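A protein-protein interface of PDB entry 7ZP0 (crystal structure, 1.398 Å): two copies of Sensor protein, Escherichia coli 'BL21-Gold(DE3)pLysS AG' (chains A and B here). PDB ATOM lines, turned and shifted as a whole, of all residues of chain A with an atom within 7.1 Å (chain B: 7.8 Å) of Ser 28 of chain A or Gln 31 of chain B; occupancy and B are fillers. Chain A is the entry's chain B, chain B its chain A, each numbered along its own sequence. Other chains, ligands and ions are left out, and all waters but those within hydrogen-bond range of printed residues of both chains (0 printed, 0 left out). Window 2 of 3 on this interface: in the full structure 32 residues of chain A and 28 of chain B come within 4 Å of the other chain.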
ATOM      1  N   ILE A  23      -8.530 -10.697   7.499  1.00  0.00           N
ATOM      2  CA  ILE A  23      -9.670 -11.577   7.718  1.00  0.00           C
ATOM      3  C   ILE A  23      -9.297 -13.028   7.424  1.00  0.00           C
ATOM      4  O   ILE A  23      -9.624 -13.931   8.201  1.00  0.00           O
ATOM      5  CB  ILE A  23     -10.876 -11.166   6.844  1.00  0.00           C
ATOM      6  CG1 ILE A  23     -11.540  -9.912   7.412  1.00  0.00           C
ATOM      7  CG2 ILE A  23     -11.898 -12.294   6.756  1.00  0.00           C
ATOM      8  CD1 ILE A  23     -12.717  -9.425   6.598  1.00  0.00           C
ATOM      9  N   ALA A  24      -8.600 -13.244   6.309  1.00  0.00           N
ATOM     10  CA  ALA A  24      -8.194 -14.585   5.897  1.00  0.00           C
ATOM     11  C   ALA A  24      -7.327 -15.272   6.955  1.00  0.00           C
ATOM     12  O   ALA A  24      -7.467 -16.472   7.211  1.00  0.00           O
ATOM     13  CB  ALA A  24      -7.451 -14.526   4.567  1.00  0.00           C
ATOM     14  N   LEU A  25      -6.440 -14.503   7.572  1.00  0.00           N
ATOM     15  CA  LEU A  25      -5.482 -15.056   8.519  1.00  0.00           C
ATOM     16  C   LEU A  25      -6.031 -15.176   9.936  1.00  0.00           C
ATOM     17  O   LEU A  25      -5.389 -15.766  10.798  1.00  0.00           O
ATOM     18  CB  LEU A  25      -4.215 -14.205   8.533  1.00  0.00           C
ATOM     19  CG  LEU A  25      -3.452 -14.175   7.213  1.00  0.00           C
ATOM     20  CD1 LEU A  25      -2.223 -13.287   7.330  1.00  0.00           C
ATOM     21  CD2 LEU A  25      -3.073 -15.590   6.812  1.00  0.00           C
ATOM     22  N   SER A  26      -7.215 -14.620  10.174  1.00  0.00           N
ATOM     23  CA  SER A  26      -7.798 -14.641  11.512  1.00  0.00           C
ATOM     24  C   SER A  26      -8.416 -15.998  11.837  1.00  0.00           C
ATOM     25  O   SER A  26      -8.549 -16.361  13.006  1.00  0.00           O
ATOM     26  CB  SER A  26      -8.851 -13.544  11.660  1.00  0.00           C
ATOM     27  OG  SER A  26     -10.056 -13.910  11.014  1.00  0.00           O
ATOM     28  N   GLN A  27      -8.798 -16.742  10.804  1.00  0.00           N
ATOM     29  CA  GLN A  27      -9.399 -18.058  10.997  1.00  0.00           C
ATOM     30  C   GLN A  27      -8.593 -19.154  10.312  1.00  0.00           C
ATOM     31  O   GLN A  27      -7.789 -18.883   9.420  1.00  0.00           O
ATOM     32  CB  GLN A  27     -10.836 -18.075  10.475  1.00  0.00           C
ATOM     33  CG  GLN A  27     -11.676 -16.900  10.942  1.00  0.00           C
ATOM     34  CD  GLN A  27     -11.622 -16.707  12.445  1.00  0.00           C
ATOM     35  OE1 GLN A  27     -11.792 -17.656  13.212  1.00  0.00           O
ATOM     36  NE2 GLN A  27     -11.381 -15.474  12.874  1.00  0.00           N
ATOM     37  N   SER A  28      -8.812 -20.393  10.740  1.00  0.00           N
ATOM     38  CA  SER A  28      -8.162 -21.540  10.121  1.00  0.00           C
ATOM     39  C   SER A  28      -8.865 -21.900   8.820  1.00  0.00           C
ATOM     40  O   SER A  28     -10.027 -22.309   8.823  1.00  0.00           O
ATOM     41  CB  SER A  28      -8.154 -22.740  11.067  1.00  0.00           C
ATOM     42  OG  SER A  28      -8.085 -23.953  10.338  1.00  0.00           O
ATOM     43  N   ARG A  29      -8.156 -21.749   7.709  1.00  0.00           N
ATOM     44  CA  ARG A  29      -8.748 -21.981   6.399  1.00  0.00           C
ATOM     45  C   ARG A  29      -8.145 -23.196   5.720  1.00  0.00           C
ATOM     46  O   ARG A  29      -7.007 -23.573   5.997  1.00  0.00           O
ATOM     47  CB  ARG A  29      -8.564 -20.752   5.509  1.00  0.00           C
ATOM     48  CG  ARG A  29      -8.899 -19.452   6.196  1.00  0.00           C
ATOM     49  CD  ARG A  29      -9.899 -18.647   5.400  1.00  0.00           C
ATOM     50  NE  ARG A  29     -10.301 -17.450   6.127  1.00  0.00           N
ATOM     51  CZ  ARG A  29     -11.321 -17.403   6.976  1.00  0.00           C
ATOM     52  NH1 ARG A  29     -11.616 -16.271   7.600  1.00  0.00           N
ATOM     53  NH2 ARG A  29     -12.046 -18.491   7.203  1.00  0.00           N
ATOM     54  N   SER A  30      -8.909 -23.801   4.820  1.00  0.00           N
ATOM     55  CA  SER A  30      -8.389 -24.880   3.997  1.00  0.00           C
ATOM     56  C   SER A  30      -7.280 -24.339   3.102  1.00  0.00           C
ATOM     57  O   SER A  30      -7.080 -23.123   3.004  1.00  0.00           O
ATOM     58  CB  SER A  30      -9.497 -25.508   3.151  1.00  0.00           C
ATOM     59  OG  SER A  30      -9.863 -24.653   2.083  1.00  0.00           O
ATOM     60  N   GLN A  31      -6.560 -25.242   2.446  1.00  0.00           N
ATOM     61  CA  GLN A  31      -5.465 -24.844   1.576  1.00  0.00           C
ATOM     62  C   GLN A  31      -5.986 -24.058   0.373  1.00  0.00           C
ATOM     63  O   GLN A  31      -5.375 -23.078  -0.045  1.00  0.00           O
ATOM     64  CB  GLN A  31      -4.675 -26.071   1.120  1.00  0.00           C
ATOM     65  CG  GLN A  31      -3.330 -25.759   0.487  1.00  0.00           C
ATOM     66  CD  GLN A  31      -3.439 -25.312  -0.960  1.00  0.00           C
ATOM     67  OE1 GLN A  31      -4.422 -25.606  -1.639  1.00  0.00           O
ATOM     68  NE2 GLN A  31      -2.428 -24.596  -1.436  1.00  0.00           N
ATOM     69  N   GLU A  33      -8.915 -22.411   0.159  1.00  0.00           N
ATOM     70  CA  GLU A  33      -9.485 -21.147   0.621  1.00  0.00           C
ATOM     71  C   GLU A  33      -8.402 -20.076   0.641  1.00  0.00           C
ATOM     72  O   GLU A  33      -8.622 -18.936   0.221  1.00  0.00           O
ATOM     73  CB  GLU A  33     -10.113 -21.296   2.012  1.00  0.00           C
ATOM     74  CG  GLU A  33     -11.476 -21.969   2.013  1.00  0.00           C
ATOM     75  CD  GLU A  33     -12.133 -21.969   3.382  1.00  0.00           C
ATOM     76  OE1 GLU A  33     -11.422 -21.768   4.388  1.00  0.00           O
ATOM     77  OE2 GLU A  33     -13.364 -22.171   3.450  1.00  0.00           O
ATOM     78  N   LEU A  34      -7.224 -20.461   1.122  1.00  0.00           N
ATOM     79  CA  LEU A  34      -6.081 -19.561   1.185  1.00  0.00           C
ATOM     80  C   LEU A  34      -5.572 -19.210  -0.211  1.00  0.00           C
ATOM     81  O   LEU A  34      -5.124 -18.088  -0.449  1.00  0.00           O
ATOM     82  CB  LEU A  34      -4.964 -20.182   2.028  1.00  0.00           C
ATOM     83  CG  LEU A  34      -5.317 -20.388   3.506  1.00  0.00           C
ATOM     84  CD1 LEU A  34      -4.232 -21.166   4.240  1.00  0.00           C
ATOM     85  CD2 LEU A  34      -5.564 -19.050   4.185  1.00  0.00           C
ATOM     86  N   SER B  28       1.671 -26.407  -5.497  1.00  0.00           N
ATOM     87  CA  SER B  28       0.733 -26.827  -4.462  1.00  0.00           C
ATOM     88  C   SER B  28       1.438 -26.859  -3.107  1.00  0.00           C
ATOM     89  O   SER B  28       2.199 -27.783  -2.818  1.00  0.00           O
ATOM     90  CB  SER B  28       0.144 -28.203  -4.789  1.00  0.00           C
ATOM     91  OG  SER B  28      -0.546 -28.188  -6.028  1.00  0.00           O
ATOM     92  N   ARG B  29       1.181 -25.849  -2.280  1.00  0.00           N
ATOM     93  CA  ARG B  29       1.881 -25.705  -1.004  1.00  0.00           C
ATOM     94  C   ARG B  29       1.007 -26.004   0.209  1.00  0.00           C
ATOM     95  O   ARG B  29      -0.219 -26.060   0.114  1.00  0.00           O
ATOM     96  CB  ARG B  29       2.454 -24.296  -0.896  1.00  0.00           C
ATOM     97  CG  ARG B  29       3.595 -24.039  -1.854  1.00  0.00           C
ATOM     98  CD  ARG B  29       4.003 -22.587  -1.812  1.00  0.00           C
ATOM     99  NE  ARG B  29       5.130 -22.316  -2.697  1.00  0.00           N
ATOM    100  CZ  ARG B  29       5.029 -22.161  -4.014  1.00  0.00           C
ATOM    101  NH1 ARG B  29       3.853 -22.313  -4.609  1.00  0.00           N
ATOM    102  NH2 ARG B  29       6.109 -21.894  -4.740  1.00  0.00           N
ATOM    103  N   SER B  30       1.659 -26.197   1.351  1.00  0.00           N
ATOM    104  CA  SER B  30       0.967 -26.538   2.587  1.00  0.00           C
ATOM    105  C   SER B  30       0.115 -25.376   3.081  1.00  0.00           C
ATOM    106  O   SER B  30       0.299 -24.233   2.659  1.00  0.00           O
ATOM    107  CB  SER B  30       1.970 -26.947   3.670  1.00  0.00           C
ATOM    108  OG  SER B  30       2.648 -25.818   4.193  1.00  0.00           O
ATOM    109  N   GLN B  31      -0.823 -25.678   3.973  1.00  0.00           N
ATOM    110  CA  GLN B  31      -1.642 -24.649   4.593  1.00  0.00           C
ATOM    111  C   GLN B  31      -0.758 -23.721   5.417  1.00  0.00           C
ATOM    112  O   GLN B  31      -1.032 -22.528   5.527  1.00  0.00           O
ATOM    113  CB  GLN B  31      -2.732 -25.274   5.470  1.00  0.00           C
ATOM    114  CG  GLN B  31      -3.614 -24.259   6.190  1.00  0.00           C
ATOM    115  CD  GLN B  31      -4.577 -24.907   7.167  1.00  0.00           C
ATOM    116  OE1 GLN B  31      -4.707 -26.131   7.212  1.00  0.00           O
ATOM    117  NE2 GLN B  31      -5.262 -24.085   7.952  1.00  0.00           N
ATOM    118  N   LYS B  32       0.313 -24.277   5.977  1.00  0.00           N
ATOM    119  CA  LYS B  32       1.244 -23.506   6.794  1.00  0.00           C
ATOM    120  C   LYS B  32       2.110 -22.591   5.934  1.00  0.00           C
ATOM    121  O   LYS B  32       2.377 -21.440   6.300  1.00  0.00           O
ATOM    122  CB  LYS B  32       2.127 -24.441   7.620  1.00  0.00           C
ATOM    123  CG  LYS B  32       2.946 -23.730   8.677  1.00  0.00           C
ATOM    124  CD  LYS B  32       2.081 -23.365   9.870  1.00  0.00           C
ATOM    125  CE  LYS B  32       2.736 -22.281  10.699  1.00  0.00           C
ATOM    126  NZ  LYS B  32       4.179 -22.576  10.908  1.00  0.00           N
ATOM    127  N   GLU B  33       2.546 -23.108   4.789  1.00  0.00           N
ATOM    128  CA  GLU B  33       3.332 -22.325   3.842  1.00  0.00           C
ATOM    129  C   GLU B  33       2.546 -21.112   3.338  1.00  0.00           C
ATOM    130  O   GLU B  33       3.081 -20.000   3.266  1.00  0.00           O
ATOM    131  CB  GLU B  33       3.780 -23.197   2.661  1.00  0.00           C
ATOM    132  CG  GLU B  33       5.120 -23.896   2.879  1.00  0.00           C
ATOM    133  CD  GLU B  33       5.323 -25.110   1.980  1.00  0.00           C
ATOM    134  OE1 GLU B  33       6.481 -25.563   1.850  1.00  0.00           O
ATOM    135  OE2 GLU B  33       4.332 -25.618   1.410  1.00  0.00           O
ATOM    136  N   LEU B  34       1.276 -21.324   3.000  1.00  0.00           N
ATOM    137  CA  LEU B  34       0.430 -20.244   2.495  1.00  0.00           C
ATOM    138  C   LEU B  34       0.132 -19.205   3.566  1.00  0.00           C
ATOM    139  O   LEU B  34       0.011 -18.016   3.263  1.00  0.00           O
ATOM    140  CB  LEU B  34      -0.881 -20.795   1.936  1.00  0.00           C
ATOM    141  CG  LEU B  34      -0.793 -21.552   0.612  1.00  0.00           C
ATOM    142  CD1 LEU B  34      -2.175 -21.692   0.010  1.00  0.00           C
ATOM    143  CD2 LEU B  34       0.134 -20.832  -0.350  1.00  0.00           C
ATOM    144  N   GLU B  35      -0.001 -19.650   4.812  1.00  0.00           N
ATOM    145  CA  GLU B  35      -0.156 -18.721   5.927  1.00  0.00           C
ATOM    146  C   GLU B  35       1.029 -17.770   5.982  1.00  0.00           C
ATOM    147  O   GLU B  35       0.859 -16.554   6.063  1.00  0.00           O
ATOM    148  CB  GLU B  35      -0.284 -19.467   7.255  1.00  0.00           C
ATOM    149  CG  GLU B  35      -1.628 -20.123   7.476  1.00  0.00           C
ATOM    150  CD  GLU B  35      -1.698 -20.858   8.799  1.00  0.00           C
ATOM    151  OE1 GLU B  35      -0.983 -20.454   9.741  1.00  0.00           O
ATOM    152  OE2 GLU B  35      -2.463 -21.839   8.894  1.00  0.00           O
ATOM    153  N   ASP B  36       2.229 -18.338   5.920  1.00  0.00           N
ATOM    154  CA  ASP B  36       3.454 -17.559   6.024  1.00  0.00           C
ATOM    155  C   ASP B  36       3.611 -16.583   4.864  1.00  0.00           C
ATOM    156  O   ASP B  36       4.207 -15.518   5.019  1.00  0.00           O
ATOM    157  CB  ASP B  36       4.664 -18.490   6.106  1.00  0.00           C
ATOM    158  CG  ASP B  36       4.762 -19.198   7.450  1.00  0.00           C
ATOM    159  OD1 ASP B  36       3.772 -19.171   8.211  1.00  0.00           O
ATOM    160  OD2 ASP B  36       5.829 -19.778   7.742  1.00  0.00           O
ATOM    161  N   VAL B  37       3.063 -16.942   3.709  1.00  0.00           N
ATOM    162  CA  VAL B  37       3.089 -16.065   2.546  1.00  0.00           C
ATOM    163  C   VAL B  37       2.166 -14.871   2.771  1.00  0.00           C
ATOM    164  O   VAL B  37       2.553 -13.724   2.556  1.00  0.00           O
ATOM    165  CB  VAL B  37       2.671 -16.816   1.258  1.00  0.00           C
ATOM    166  CG1 VAL B  37       2.466 -15.841   0.103  1.00  0.00           C
ATOM    167  CG2 VAL B  37       3.700 -17.881   0.901  1.00  0.00           C
ATOM    168  N   LEU B  38       0.948 -15.150   3.222  1.00  0.00           N
ATOM    169  CA  LEU B  38      -0.049 -14.113   3.460  1.00  0.00           C
ATOM    170  C   LEU B  38       0.360 -13.178   4.591  1.00  0.00           C
ATOM    171  O   LEU B  38       0.101 -11.979   4.523  1.00  0.00           O
ATOM    172  CB  LEU B  38      -1.410 -14.743   3.763  1.00  0.00           C
ATOM    173  CG  LEU B  38      -2.197 -15.271   2.561  1.00  0.00           C
ATOM    174  CD1 LEU B  38      -3.556 -15.807   2.991  1.00  0.00           C
ATOM    175  CD2 LEU B  38      -2.368 -14.182   1.515  1.00  0.00           C
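O of Arg 29 of chain B sits at hydrogen-bond distance from NE2 of Gln 31 of chain A (3.1 Å). NE2 of Gln 31 of chain B lies within hydrogen-bond range of O of Arg 29 of chain A (2.7 Å).
The backbone carbonyl oxygen (O) of Ala 24 of chain A lies within hydrogen-bond range of the guanidinium group (NE) of Arg 29 of chain A. O of Ile 23 of chain A is in hydrogen-bond range of NH1 of Arg 29 of chain A, at 3.1 Å.
Among the printed residues, pairs that only touch across the chains: Leu 25 of chain A with Leu 38 of chain B, Ser 28 of chain A with Gln 31 of chain B, Gln 31 of chain A with Leu 34 of chain B, Leu 34 of chain A with Gln 31 of chain B, Leu 34 of chain A with Leu 34 of chain B and Leu 34 of chain A with Leu 38 of chain B.
Ser 28 of chain A touches one residue of chain B. Of the printed residues of chain A, Gln 31 of chain B touches Ser 28, Arg 29 and Leu 34. Of the printed residues of chain A, Arg 29 of chain B touches Gln 31 (3.1 Å). Printed residues of chain B within 4 Å of Leu 25 of chain A: Leu 38. Ser 30 of chain A touches none of the printed residues of chain B. The nearest residue of chain B that does not touch Ser 28 of chain A is Glu 35 of chain B (5.8 Å).
Printed residues of chain B that touch a printed residue of chain A: Arg 29, Gln 31, Leu 34 and Leu 38. Along chain A the printed residues that touch a printed residue of chain B span positions 25 to 34. Among the printed residues, no Asp or Glu carboxylate lies within 4 Å of a Lys or Arg side-chain nitrogen of the other chain.
Ser 28 of chain A touches Gln 31 of chain B, but with the chains exchanged Gln 31 of chain A does not touch Ser 28 of chain B (4.8 Å). Arg 29 of chain A touches Gln 31 of chain B, and with the chains exchanged Gln 31 of chain A touches Arg 29 of chain B. Gln 31 of chain A touches Leu 34 of chain B, and with the chains exchanged Leu 34 of chain A touches Gln 31 of chain B. Leu 34 of chain B touches its own counterpart, Leu 34 of chain A. Of the 8 pairs that touch across the chains among the printed residues, 5 have their exchanged pair printed and touching as well.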
